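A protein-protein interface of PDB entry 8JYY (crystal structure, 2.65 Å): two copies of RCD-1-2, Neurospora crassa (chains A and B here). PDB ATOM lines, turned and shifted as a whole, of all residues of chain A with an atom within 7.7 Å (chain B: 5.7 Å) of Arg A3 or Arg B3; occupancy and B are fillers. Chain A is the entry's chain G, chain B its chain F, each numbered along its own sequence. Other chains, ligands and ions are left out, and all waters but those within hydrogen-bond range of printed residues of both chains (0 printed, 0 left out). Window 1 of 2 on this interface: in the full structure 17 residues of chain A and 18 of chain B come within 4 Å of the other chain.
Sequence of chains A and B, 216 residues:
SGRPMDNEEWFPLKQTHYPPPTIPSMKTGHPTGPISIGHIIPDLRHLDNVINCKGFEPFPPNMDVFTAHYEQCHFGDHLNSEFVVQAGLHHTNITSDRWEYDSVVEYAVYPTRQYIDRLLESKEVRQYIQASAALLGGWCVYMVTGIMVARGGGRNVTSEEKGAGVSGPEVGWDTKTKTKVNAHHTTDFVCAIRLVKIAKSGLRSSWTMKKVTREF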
ATOM      1  N   SER A   1       7.849 -17.055   5.777  1.00  0.00           N
ATOM      2  CA  SER A   1       8.746 -16.439   6.745  1.00  0.00           C
ATOM      3  C   SER A   1      10.190 -16.892   6.535  1.00  0.00           C
ATOM      4  O   SER A   1      11.073 -16.567   7.330  1.00  0.00           O
ATOM      5  CB  SER A   1       8.292 -16.758   8.170  1.00  0.00           C
ATOM      6  OG  SER A   1       7.003 -16.227   8.422  1.00  0.00           O
ATOM      7  N   GLY A   2      10.420 -17.640   5.457  1.00  0.00           N
ATOM      8  CA  GLY A   2      11.749 -18.088   5.097  1.00  0.00           C
ATOM      9  C   GLY A   2      12.352 -18.998   6.151  1.00  0.00           C
ATOM     10  O   GLY A   2      11.660 -19.774   6.819  1.00  0.00           O
ATOM     11  N   ARG A   3      13.676 -18.900   6.303  1.00  0.00           N
ATOM     12  CA  ARG A   3      14.360 -19.678   7.321  1.00  0.00           C
ATOM     13  C   ARG A   3      14.174 -19.034   8.693  1.00  0.00           C
ATOM     14  O   ARG A   3      14.076 -17.808   8.803  1.00  0.00           O
ATOM     15  CB  ARG A   3      15.850 -19.791   7.006  1.00  0.00           C
ATOM     16  CG  ARG A   3      16.163 -20.206   5.579  1.00  0.00           C
ATOM     17  CD  ARG A   3      17.589 -20.721   5.450  1.00  0.00           C
ATOM     18  NE  ARG A   3      17.670 -22.163   5.653  1.00  0.00           N
ATOM     19  CZ  ARG A   3      17.739 -23.054   4.673  1.00  0.00           C
ATOM     20  NH1 ARG A   3      17.762 -22.684   3.403  1.00  0.00           N
ATOM     21  NH2 ARG A   3      17.792 -24.348   4.975  1.00  0.00           N
ATOM     22  N   PRO A   4      14.114 -19.840   9.752  1.00  0.00           N
ATOM     23  CA  PRO A   4      13.943 -19.275  11.096  1.00  0.00           C
ATOM     24  C   PRO A   4      15.120 -18.396  11.485  1.00  0.00           C
ATOM     25  O   PRO A   4      16.239 -18.556  10.990  1.00  0.00           O
ATOM     26  CB  PRO A   4      13.853 -20.515  11.995  1.00  0.00           C
ATOM     27  CG  PRO A   4      13.466 -21.630  11.078  1.00  0.00           C
ATOM     28  CD  PRO A   4      14.106 -21.311   9.764  1.00  0.00           C
ATOM     29  N   MET A   5      14.853 -17.449  12.385  1.00  0.00           N
ATOM     30  CA  MET A   5      15.899 -16.578  12.904  1.00  0.00           C
ATOM     31  C   MET A   5      16.719 -17.235  14.006  1.00  0.00           C
ATOM     32  O   MET A   5      17.713 -16.648  14.446  1.00  0.00           O
ATOM     33  CB  MET A   5      15.287 -15.279  13.431  1.00  0.00           C
ATOM     34  CG  MET A   5      14.450 -14.524  12.416  1.00  0.00           C
ATOM     35  SD  MET A   5      15.431 -13.760  11.112  1.00  0.00           S
ATOM     36  CE  MET A   5      16.440 -12.632  12.069  1.00  0.00           C
ATOM     37  N   ASP A   6      16.333 -18.430  14.457  1.00  0.00           N
ATOM     38  CA  ASP A   6      17.036 -19.129  15.533  1.00  0.00           C
ATOM     39  C   ASP A   6      18.225 -19.899  14.959  1.00  0.00           C
ATOM     40  O   ASP A   6      18.271 -21.131  14.944  1.00  0.00           O
ATOM     41  CB  ASP A   6      16.091 -20.062  16.276  1.00  0.00           C
ATOM     42  CG  ASP A   6      14.921 -19.336  16.892  1.00  0.00           C
ATOM     43  OD1 ASP A   6      15.097 -18.175  17.316  1.00  0.00           O
ATOM     44  OD2 ASP A   6      13.825 -19.931  16.953  1.00  0.00           O
ATOM     45  N   ASN A   7      19.204 -19.142  14.475  1.00  0.00           N
ATOM     46  CA  ASN A   7      20.445 -19.761  14.042  1.00  0.00           C
ATOM     47  C   ASN A   7      21.204 -20.315  15.244  1.00  0.00           C
ATOM     48  O   ASN A   7      20.924 -19.983  16.399  1.00  0.00           O
ATOM     49  CB  ASN A   7      21.317 -18.763  13.280  1.00  0.00           C
ATOM     50  CG  ASN A   7      20.994 -18.722  11.801  1.00  0.00           C
ATOM     51  OD1 ASN A   7      20.904 -17.652  11.201  1.00  0.00           O
ATOM     52  ND2 ASN A   7      20.816 -19.895  11.205  1.00  0.00           N
ATOM     53  N   GLU A   8      22.181 -21.176  14.955  1.00  0.00           N
ATOM     54  CA  GLU A   8      22.970 -21.787  16.018  1.00  0.00           C
ATOM     55  C   GLU A   8      23.758 -20.756  16.815  1.00  0.00           C
ATOM     56  O   GLU A   8      24.176 -21.047  17.940  1.00  0.00           O
ATOM     57  CB  GLU A   8      23.922 -22.828  15.430  1.00  0.00           C
ATOM     58  CG  GLU A   8      24.986 -22.245  14.516  1.00  0.00           C
ATOM     59  CD  GLU A   8      25.827 -23.313  13.846  1.00  0.00           C
ATOM     60  OE1 GLU A   8      25.264 -24.360  13.463  1.00  0.00           O
ATOM     61  OE2 GLU A   8      27.050 -23.107  13.707  1.00  0.00           O
ATOM     62  N   GLU A   9      23.959 -19.562  16.265  1.00  0.00           N
ATOM     63  CA  GLU A   9      24.725 -18.511  16.918  1.00  0.00           C
ATOM     64  C   GLU A   9      23.853 -17.507  17.661  1.00  0.00           C
ATOM     65  O   GLU A   9      24.385 -16.547  18.226  1.00  0.00           O
ATOM     66  CB  GLU A   9      25.589 -17.781  15.885  1.00  0.00           C
ATOM     67  CG  GLU A   9      24.845 -17.434  14.605  1.00  0.00           C
ATOM     68  CD  GLU A   9      25.767 -16.947  13.505  1.00  0.00           C
ATOM     69  OE1 GLU A   9      26.857 -16.429  13.823  1.00  0.00           O
ATOM     70  OE2 GLU A   9      25.403 -17.092  12.318  1.00  0.00           O
ATOM     71  N   TRP A  10      22.536 -17.705  17.686  1.00  0.00           N
ATOM     72  CA  TRP A  10      21.609 -16.773  18.323  1.00  0.00           C
ATOM     73  C   TRP A  10      20.790 -17.519  19.369  1.00  0.00           C
ATOM     74  O   TRP A  10      19.930 -18.337  19.024  1.00  0.00           O
ATOM     75  CB  TRP A  10      20.701 -16.112  17.288  1.00  0.00           C
ATOM     76  CG  TRP A  10      21.410 -15.112  16.432  1.00  0.00           C
ATOM     77  CD1 TRP A  10      21.950 -15.324  15.198  1.00  0.00           C
ATOM     78  CD2 TRP A  10      21.664 -13.739  16.750  1.00  0.00           C
ATOM     79  NE1 TRP A  10      22.521 -14.168  14.726  1.00  0.00           N
ATOM     80  CE2 TRP A  10      22.360 -13.179  15.660  1.00  0.00           C
ATOM     81  CE3 TRP A  10      21.370 -12.927  17.851  1.00  0.00           C
ATOM     82  CZ2 TRP A  10      22.765 -11.846  15.639  1.00  0.00           C
ATOM     83  CZ3 TRP A  10      21.773 -11.604  17.827  1.00  0.00           C
ATOM     84  CH2 TRP A  10      22.463 -11.077  16.728  1.00  0.00           C
ATOM     85  N   ALA A  68      21.248  -5.192  10.626  1.00  0.00           N
ATOM     86  CA  ALA A  68      20.693  -6.054   9.585  1.00  0.00           C
ATOM     87  C   ALA A  68      19.196  -6.189   9.817  1.00  0.00           C
ATOM     88  O   ALA A  68      18.776  -6.621  10.893  1.00  0.00           O
ATOM     89  CB  ALA A  68      21.369  -7.426   9.582  1.00  0.00           C
ATOM     90  N   TYR A  70      15.313  -7.624   8.873  1.00  0.00           N
ATOM     91  CA  TYR A  70      14.588  -8.757   8.320  1.00  0.00           C
ATOM     92  C   TYR A  70      13.098  -8.525   8.524  1.00  0.00           C
ATOM     93  O   TYR A  70      12.684  -7.861   9.479  1.00  0.00           O
ATOM     94  CB  TYR A  70      15.010 -10.081   8.974  1.00  0.00           C
ATOM     95  CG  TYR A  70      16.493 -10.380   8.923  1.00  0.00           C
ATOM     96  CD1 TYR A  70      17.369  -9.815   9.842  1.00  0.00           C
ATOM     97  CD2 TYR A  70      17.015 -11.243   7.968  1.00  0.00           C
ATOM     98  CE1 TYR A  70      18.722 -10.089   9.803  1.00  0.00           C
ATOM     99  CE2 TYR A  70      18.368 -11.524   7.922  1.00  0.00           C
ATOM    100  CZ  TYR A  70      19.216 -10.944   8.841  1.00  0.00           C
ATOM    101  OH  TYR A  70      20.562 -11.223   8.796  1.00  0.00           O
ATOM    102  N   GLU A  71      12.292  -9.083   7.622  1.00  0.00           N
ATOM    103  CA  GLU A  71      10.856  -8.841   7.610  1.00  0.00           C
ATOM    104  C   GLU A  71      10.098 -10.160   7.569  1.00  0.00           C
ATOM    105  O   GLU A  71      10.533 -11.115   6.920  1.00  0.00           O
ATOM    106  CB  GLU A  71      10.461  -7.969   6.413  1.00  0.00           C
ATOM    107  CG  GLU A  71      11.238  -6.667   6.329  1.00  0.00           C
ATOM    108  CD  GLU A  71      10.919  -5.872   5.081  1.00  0.00           C
ATOM    109  OE1 GLU A  71      10.055  -6.315   4.296  1.00  0.00           O
ATOM    110  OE2 GLU A  71      11.534  -4.803   4.884  1.00  0.00           O
ATOM    111  N   GLN A  72       8.958 -10.193   8.260  1.00  0.00           N
ATOM    112  CA  GLN A  72       8.111 -11.381   8.375  1.00  0.00           C
ATOM    113  C   GLN A  72       8.928 -12.595   8.816  1.00  0.00           C
ATOM    114  O   GLN A  72       9.041 -13.600   8.114  1.00  0.00           O
ATOM    115  CB  GLN A  72       7.367 -11.660   7.065  1.00  0.00           C
ATOM    116  CG  GLN A  72       6.280 -10.648   6.737  1.00  0.00           C
ATOM    117  CD  GLN A  72       5.337 -11.137   5.655  1.00  0.00           C
ATOM    118  OE1 GLN A  72       5.480 -12.250   5.148  1.00  0.00           O
ATOM    119  NE2 GLN A  72       4.365 -10.307   5.297  1.00  0.00           N
ATOM    120  N   CYS A  73       9.501 -12.481  10.008  1.00  0.00           N
ATOM    121  CA  CYS A  73      10.383 -13.498  10.560  1.00  0.00           C
ATOM    122  C   CYS A  73       9.615 -14.423  11.498  1.00  0.00           C
ATOM    123  O   CYS A  73       8.452 -14.190  11.831  1.00  0.00           O
ATOM    124  CB  CYS A  73      11.548 -12.839  11.299  1.00  0.00           C
ATOM    125  SG  CYS A  73      12.217 -11.397  10.458  1.00  0.00           S
ATOM    126  N   HIS A  74      10.291 -15.485  11.929  1.00  0.00           N
ATOM    127  CA  HIS A  74       9.687 -16.426  12.863  1.00  0.00           C
ATOM    128  C   HIS A  74      10.784 -17.154  13.624  1.00  0.00           C
ATOM    129  O   HIS A  74      11.936 -17.220  13.186  1.00  0.00           O
ATOM    130  CB  HIS A  74       8.772 -17.427  12.145  1.00  0.00           C
ATOM    131  CG  HIS A  74       9.505 -18.514  11.423  1.00  0.00           C
ATOM    132  ND1 HIS A  74      10.177 -18.303  10.239  1.00  0.00           N
ATOM    133  CD2 HIS A  74       9.662 -19.828  11.714  1.00  0.00           C
ATOM    134  CE1 HIS A  74      10.718 -19.438   9.832  1.00  0.00           C
ATOM    135  NE2 HIS A  74      10.421 -20.378  10.711  1.00  0.00           N
ATOM    136  N   PHE A  75      10.405 -17.694  14.779  1.00  0.00           N
ATOM    137  CA  PHE A  75      11.283 -18.494  15.617  1.00  0.00           C
ATOM    138  C   PHE A  75      10.848 -19.952  15.584  1.00  0.00           C
ATOM    139  O   PHE A  75       9.659 -20.260  15.469  1.00  0.00           O
ATOM    140  CB  PHE A  75      11.277 -17.997  17.068  1.00  0.00           C
ATOM    141  CG  PHE A  75      12.233 -16.871  17.331  1.00  0.00           C
ATOM    142  CD1 PHE A  75      12.866 -16.217  16.288  1.00  0.00           C
ATOM    143  CD2 PHE A  75      12.510 -16.476  18.629  1.00  0.00           C
ATOM    144  CE1 PHE A  75      13.748 -15.184  16.536  1.00  0.00           C
ATOM    145  CE2 PHE A  75      13.392 -15.445  18.883  1.00  0.00           C
ATOM    146  CZ  PHE A  75      14.013 -14.798  17.835  1.00  0.00           C
ATOM    147  N   GLY A  76      11.820 -20.851  15.697  1.00  0.00           N
ATOM    148  CA  GLY A  76      11.512 -22.267  15.706  1.00  0.00           C
ATOM    149  C   GLY A  76      12.713 -23.157  15.939  1.00  0.00           C
ATOM    150  O   GLY A  76      13.722 -23.050  15.235  1.00  0.00           O
ATOM    151  N   VAL A 104      12.537  -7.724  12.381  1.00  0.00           N
ATOM    152  CA  VAL A 104      13.571  -8.066  13.349  1.00  0.00           C
ATOM    153  C   VAL A 104      14.874  -7.415  12.909  1.00  0.00           C
ATOM    154  O   VAL A 104      15.296  -7.573  11.760  1.00  0.00           O
ATOM    155  CB  VAL A 104      13.750  -9.589  13.492  1.00  0.00           C
ATOM    156  CG1 VAL A 104      14.927  -9.895  14.399  1.00  0.00           C
ATOM    157  CG2 VAL A 104      12.484 -10.223  14.038  1.00  0.00           C
ATOM    158  N   GLU A 106      18.938  -7.003  13.732  1.00  0.00           N
ATOM    159  CA  GLU A 106      20.151  -7.440  14.405  1.00  0.00           C
ATOM    160  C   GLU A 106      21.107  -6.263  14.524  1.00  0.00           C
ATOM    161  O   GLU A 106      21.372  -5.573  13.533  1.00  0.00           O
ATOM    162  CB  GLU A 106      20.839  -8.570  13.636  1.00  0.00           C
ATOM    163  CG  GLU A 106      19.954  -9.731  13.245  1.00  0.00           C
ATOM    164  CD  GLU A 106      20.751 -10.888  12.671  1.00  0.00           C
ATOM    165  OE1 GLU A 106      21.967 -10.716  12.434  1.00  0.00           O
ATOM    166  OE2 GLU A 106      20.163 -11.969  12.458  1.00  0.00           O
ATOM    167  N   MET A 148      19.173  -9.111  18.925  1.00  0.00           N
ATOM    168  CA  MET A 148      18.072  -9.082  17.973  1.00  0.00           C
ATOM    169  C   MET A 148      16.866  -8.464  18.664  1.00  0.00           C
ATOM    170  O   MET A 148      16.443  -8.941  19.723  1.00  0.00           O
ATOM    171  CB  MET A 148      17.741 -10.488  17.475  1.00  0.00           C
ATOM    172  CG  MET A 148      18.172 -10.764  16.050  1.00  0.00           C
ATOM    173  SD  MET A 148      17.991 -12.497  15.585  1.00  0.00           S
ATOM    174  CE  MET A 148      16.294 -12.792  16.063  1.00  0.00           C
ATOM    175  N   ALA A 192      16.639 -12.251  20.974  1.00  0.00           N
ATOM    176  CA  ALA A 192      17.777 -13.154  20.862  1.00  0.00           C
ATOM    177  C   ALA A 192      19.061 -12.382  21.121  1.00  0.00           C
ATOM    178  O   ALA A 192      19.126 -11.165  20.937  1.00  0.00           O
ATOM    179  CB  ALA A 192      17.828 -13.828  19.486  1.00  0.00           C
ATOM    180  N   ARG A 194      23.565 -12.864  20.736  1.00  0.00           N
ATOM    181  CA  ARG A 194      24.712 -13.578  20.192  1.00  0.00           C
ATOM    182  C   ARG A 194      25.896 -13.331  21.112  1.00  0.00           C
ATOM    183  O   ARG A 194      26.297 -12.177  21.308  1.00  0.00           O
ATOM    184  CB  ARG A 194      25.030 -13.116  18.770  1.00  0.00           C
ATOM    185  CG  ARG A 194      26.195 -13.846  18.128  1.00  0.00           C
ATOM    186  CD  ARG A 194      26.618 -13.170  16.838  1.00  0.00           C
ATOM    187  NE  ARG A 194      27.234 -11.873  17.088  1.00  0.00           N
ATOM    188  CZ  ARG A 194      27.680 -11.060  16.141  1.00  0.00           C
ATOM    189  NH1 ARG A 194      27.578 -11.371  14.858  1.00  0.00           N
ATOM    190  NH2 ARG A 194      28.244  -9.907  16.488  1.00  0.00           N
ATOM    191  N   SER B   1      10.860 -13.858   2.534  1.00  0.00           N
ATOM    192  CA  SER B   1      10.962 -13.090   3.770  1.00  0.00           C
ATOM    193  C   SER B   1      11.812 -13.824   4.806  1.00  0.00           C
ATOM    194  O   SER B   1      12.318 -14.916   4.545  1.00  0.00           O
ATOM    195  CB  SER B   1       9.569 -12.800   4.334  1.00  0.00           C
ATOM    196  OG  SER B   1       8.843 -13.997   4.552  1.00  0.00           O
ATOM    197  N   GLY B   2      11.964 -13.214   5.979  1.00  0.00           N
ATOM    198  CA  GLY B   2      12.763 -13.801   7.036  1.00  0.00           C
ATOM    199  C   GLY B   2      14.221 -13.917   6.636  1.00  0.00           C
ATOM    200  O   GLY B   2      14.774 -13.073   5.924  1.00  0.00           O
ATOM    201  N   ARG B   3      14.858 -14.985   7.107  1.00  0.00           N
ATOM    202  CA  ARG B   3      16.241 -15.240   6.731  1.00  0.00           C
ATOM    203  C   ARG B   3      16.291 -15.872   5.340  1.00  0.00           C
ATOM    204  O   ARG B   3      15.477 -16.746   5.028  1.00  0.00           O
ATOM    205  CB  ARG B   3      16.915 -16.157   7.750  1.00  0.00           C
ATOM    206  CG  ARG B   3      18.310 -15.711   8.151  1.00  0.00           C
ATOM    207  CD  ARG B   3      18.514 -15.837   9.651  1.00  0.00           C
ATOM    208  NE  ARG B   3      19.656 -15.057  10.108  1.00  0.00           N
ATOM    209  CZ  ARG B   3      19.929 -14.804  11.381  1.00  0.00           C
ATOM    210  NH1 ARG B   3      19.157 -15.258  12.355  1.00  0.00           N
ATOM    211  NH2 ARG B   3      21.001 -14.079  11.684  1.00  0.00           N
ATOM    212  N   PRO B   4      17.224 -15.448   4.488  1.00  0.00           N
ATOM    213  CA  PRO B   4      17.243 -15.948   3.109  1.00  0.00           C
ATOM    214  C   PRO B   4      17.531 -17.442   3.050  1.00  0.00           C
ATOM    215  O   PRO B   4      18.168 -18.011   3.939  1.00  0.00           O
ATOM    216  CB  PRO B   4      18.364 -15.135   2.451  1.00  0.00           C
ATOM    217  CG  PRO B   4      19.242 -14.720   3.588  1.00  0.00           C
ATOM    218  CD  PRO B   4      18.318 -14.497   4.749  1.00  0.00           C
ATOM    219  N   MET B   5      17.048 -18.074   1.978  1.00  0.00           N
ATOM    220  CA  MET B   5      17.203 -19.516   1.822  1.00  0.00           C
ATOM    221  C   MET B   5      18.579 -19.898   1.291  1.00  0.00           C
ATOM    222  O   MET B   5      19.072 -20.989   1.594  1.00  0.00           O
ATOM    223  CB  MET B   5      16.124 -20.064   0.888  1.00  0.00           C
ATOM    224  CG  MET B   5      14.702 -19.811   1.350  1.00  0.00           C
ATOM    225  SD  MET B   5      14.201 -20.855   2.731  1.00  0.00           S
ATOM    226  CE  MET B   5      14.516 -22.486   2.060  1.00  0.00           C
ATOM    227  N   ASP B   6      19.208 -19.027   0.500  1.00  0.00           N
ATOM    228  CA  ASP B   6      20.508 -19.323  -0.105  1.00  0.00           C
ATOM    229  C   ASP B   6      21.624 -19.013   0.895  1.00  0.00           C
ATOM    230  O   ASP B   6      22.415 -18.080   0.743  1.00  0.00           O
ATOM    231  CB  ASP B   6      20.684 -18.548  -1.404  1.00  0.00           C
ATOM    232  CG  ASP B   6      20.424 -17.063  -1.239  1.00  0.00           C
ATOM    233  OD1 ASP B   6      19.410 -16.702  -0.606  1.00  0.00           O
ATOM    234  OD2 ASP B   6      21.238 -16.257  -1.738  1.00  0.00           O
ATOM    235  N   ASN B   7      21.680 -19.834   1.941  1.00  0.00           N
ATOM    236  CA  ASN B   7      22.721 -19.718   2.953  1.00  0.00           C
ATOM    237  C   ASN B   7      24.010 -20.348   2.425  1.00  0.00           C
ATOM    238  O   ASN B   7      24.129 -20.684   1.244  1.00  0.00           O
ATOM    239  CB  ASN B   7      22.259 -20.353   4.263  1.00  0.00           C
ATOM    240  CG  ASN B   7      21.872 -21.808   4.100  1.00  0.00           C
ATOM    241  OD1 ASN B   7      21.552 -22.255   2.999  1.00  0.00           O
ATOM    242  ND2 ASN B   7      21.891 -22.555   5.197  1.00  0.00           N
ATOM    243  N   TRP B  10      23.723 -24.052   0.765  1.00  0.00           N
ATOM    244  CA  TRP B  10      22.995 -24.288  -0.475  1.00  0.00           C
ATOM    245  C   TRP B  10      23.534 -23.385  -1.575  1.00  0.00           C
ATOM    246  O   TRP B  10      23.728 -22.184  -1.361  1.00  0.00           O
ATOM    247  CB  TRP B  10      21.494 -24.048  -0.283  1.00  0.00           C
ATOM    248  CG  TRP B  10      20.833 -25.051   0.616  1.00  0.00           C
ATOM    249  CD1 TRP B  10      20.724 -24.988   1.975  1.00  0.00           C
ATOM    250  CD2 TRP B  10      20.183 -26.264   0.217  1.00  0.00           C
ATOM    251  NE1 TRP B  10      20.050 -26.088   2.447  1.00  0.00           N
ATOM    252  CE2 TRP B  10      19.707 -26.887   1.388  1.00  0.00           C
ATOM    253  CE3 TRP B  10      19.959 -26.885  -1.016  1.00  0.00           C
ATOM    254  CZ2 TRP B  10      19.021 -28.100   1.363  1.00  0.00           C
ATOM    255  CZ3 TRP B  10      19.277 -28.091  -1.038  1.00  0.00           C
ATOM    256  CH2 TRP B  10      18.817 -28.685   0.143  1.00  0.00           C
ATOM    257  N   TYR B  70       9.087 -24.666   3.693  1.00  0.00           N
ATOM    258  CA  TYR B  70       9.248 -23.270   4.066  1.00  0.00           C
ATOM    259  C   TYR B  70       8.271 -22.428   3.260  1.00  0.00           C
ATOM    260  O   TYR B  70       8.017 -22.714   2.086  1.00  0.00           O
ATOM    261  CB  TYR B  70      10.682 -22.777   3.816  1.00  0.00           C
ATOM    262  CG  TYR B  70      11.774 -23.622   4.437  1.00  0.00           C
ATOM    263  CD1 TYR B  70      12.287 -24.730   3.771  1.00  0.00           C
ATOM    264  CD2 TYR B  70      12.309 -23.299   5.676  1.00  0.00           C
ATOM    265  CE1 TYR B  70      13.288 -25.500   4.331  1.00  0.00           C
ATOM    266  CE2 TYR B  70      13.312 -24.062   6.244  1.00  0.00           C
ATOM    267  CZ  TYR B  70      13.798 -25.161   5.567  1.00  0.00           C
ATOM    268  OH  TYR B  70      14.797 -25.923   6.129  1.00  0.00           O
ATOM    269  N   HIS B  74      12.751 -16.153   0.091  1.00  0.00           N
ATOM    270  CA  HIS B  74      13.423 -15.278  -0.856  1.00  0.00           C
ATOM    271  C   HIS B  74      14.885 -15.685  -0.968  1.00  0.00           C
ATOM    272  O   HIS B  74      15.433 -16.369  -0.100  1.00  0.00           O
ATOM    273  CB  HIS B  74      13.301 -13.801  -0.454  1.00  0.00           C
ATOM    274  CG  HIS B  74      14.144 -13.417   0.721  1.00  0.00           C
ATOM    275  ND1 HIS B  74      13.805 -13.736   2.018  1.00  0.00           N
ATOM    276  CD2 HIS B  74      15.307 -12.729   0.796  1.00  0.00           C
ATOM    277  CE1 HIS B  74      14.725 -13.265   2.841  1.00  0.00           C
ATOM    278  NE2 HIS B  74      15.648 -12.650   2.123  1.00  0.00           N
ATOM    279  N   GLU B 106      12.856 -28.423   0.745  1.00  0.00           N
ATOM    280  CA  GLU B 106      14.176 -29.035   0.731  1.00  0.00           C
ATOM    281  C   GLU B 106      14.022 -30.546   0.831  1.00  0.00           C
ATOM    282  O   GLU B 106      13.287 -31.042   1.694  1.00  0.00           O
ATOM    283  CB  GLU B 106      15.036 -28.529   1.890  1.00  0.00           C
ATOM    284  CG  GLU B 106      15.431 -27.066   1.815  1.00  0.00           C
ATOM    285  CD  GLU B 106      16.274 -26.640   3.003  1.00  0.00           C
ATOM    286  OE1 GLU B 106      16.286 -27.372   4.016  1.00  0.00           O
ATOM    287  OE2 GLU B 106      16.929 -25.580   2.924  1.00  0.00           O
ATOM    288  N   MET B 148      16.744 -28.074  -3.401  1.00  0.00           N
ATOM    289  CA  MET B 148      15.773 -27.094  -2.942  1.00  0.00           C
ATOM    290  C   MET B 148      14.907 -26.711  -4.133  1.00  0.00           C
ATOM    291  O   MET B 148      15.416 -26.175  -5.126  1.00  0.00           O
ATOM    292  CB  MET B 148      16.473 -25.869  -2.353  1.00  0.00           C
ATOM    293  CG  MET B 148      15.632 -25.098  -1.364  1.00  0.00           C
ATOM    294  SD  MET B 148      16.280 -23.460  -0.985  1.00  0.00           S
ATOM    295  CE  MET B 148      17.671 -23.877   0.057  1.00  0.00           C
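The backbone NH (N) of Ser A1 sits close to the side-chain hydroxyl (OG) of Ser B1, at 3.4 Å. N of Arg A3 sits at hydrogen-bond distance from O of Arg B3 (3.1 Å). The backbone carbonyl oxygen of Met A5 lies within hydrogen-bond range of the guanidinium group of Arg B3 (2.9 Å). NH1 of Arg A3 is in hydrogen-bond range of O of Met B5 (2.8 Å). NE1 of Trp A10 lies close to NH2 of Arg B3, at 3.4 Å. The side-chain carboxylate of Glu B106 is in salt-bridge range of the guanidinium group of Arg A3, 2.5 Å away. N of Gly A2 lies close to O of Ser B1 (3.4 Å). The guanidinium group (NE) of Arg B3 sits close to the side-chain amide oxygen (OD1) of Asn A7, 3.1 Å away. The side-chain carboxylate (OE2) of Glu A106 lies within salt-bridge range of the guanidinium group (NH1) of Arg B3 (3.4 Å). N of Gly B2 is in hydrogen-bond range of O of Glu A71.
The side-chain sulfur (SG) of Cys A73 is in hydrogen-bond range of the backbone NH (N) of Glu A71 (3.7 Å). The side-chain carboxylate of Glu B106 lies within hydrogen-bond range of the side-chain hydroxyl of Tyr B70. The backbone NH (N) of Met A5 is in hydrogen-bond range of the backbone carbonyl oxygen (O) of His A74. The backbone carbonyl oxygen (O) of His B74 is in hydrogen-bond range of the backbone NH (N) of Met B5, 3.1 Å away. The backbone carbonyl oxygen of Gln A72 lies close to the side-chain hydroxyl of Ser A1 (3.3 Å). The backbone carbonyl oxygen (O) of Tyr A70 sits close to the side-chain sulfur (SG) of Cys A73 (3.7 Å).
Gly A2 touches Arg B3. Arg A3 touches Pro B4. NH1 of Arg A3 touches OD1 of Asn B7, at 3.8 Å. Trp B10 touches Arg A3 (NE1 to NH2, 3.8 Å). NH1 of Arg A3 touches CE of Met B148, at 3.6 Å. Pro A4 touches Arg B3. Tyr A70 touches Gly B2. Glu A71 touches Ser B1 (O to CB, 3.2 Å). O of Gln A72 touches OG of Ser B1 (3.6 Å). O of Gln A72 touches N of Gly B2 (3.6 Å).
Printed residues of chain B within 4 Å of Gly A2: Ser B1, Arg B3 and Tyr B70. Of the printed residues of chain B, Gln A72 touches Ser B1 (3.6 Å) and Gly B2 (3.6 Å). His A74 touches none of the printed residues of chain B. Val A104 touches none of the printed residues of chain B. Printed residues of chain A within 4 Å of Gly B2: Ser A1, Tyr A70, Glu A71 and Gln A72. Arg B3 touches seven residues of chain A. Pro B4 touches just one residue of chain A: Arg A3 (3.2 Å). Of the printed residues of chain A, Met B5 touches Arg A3. Printed residues of chain A within 4 Å of Trp B10: Arg A3. Printed residues of chain A within 4 Å of Glu B106: Arg A3 (2.5 Å). The nearest printed residue of chain A that does not touch Arg B3 is Tyr A70 (4.1 Å). The nearest printed residue of chain A that does not touch Met B148 is Gly A2 (9.3 Å).
Of the 12 printed residues of chain B, 10 touch a printed residue of chain A. Along chain B the printed residues that touch a printed residue of chain A span positions 1 to 148. Hydrophobic or aromatic side chains of chain A within 4 Å of the printed part of chain B: Met A5, Trp A10 and Tyr A70. Among the printed residues, Asp or Glu carboxylates within 4 Å of a Lys or Arg side-chain nitrogen of the other chain: Arg A3 with Glu B106 (2.5 Å) and Glu A106 with Arg B3 (2.4 Å).
Ser B1 touches its own counterpart, Ser A1. Gly A2 touches Tyr B70, and with the chains exchanged Tyr A70 touches Gly B2. Arg A3 touches Pro B4, and with the chains exchanged Pro A4 touches Arg B3. Arg A3 touches Tyr B70, but with the chains exchanged Tyr A70 does not touch Arg B3 (4.1 Å). Positions printed for both chains: 1, 2, 3, 4, 5, 6, 7, 10, 70, 74, 106 and 148. Of the 23 pairs that touch across the chains among the printed residues, 16 have their exchanged pair printed and touching as well.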
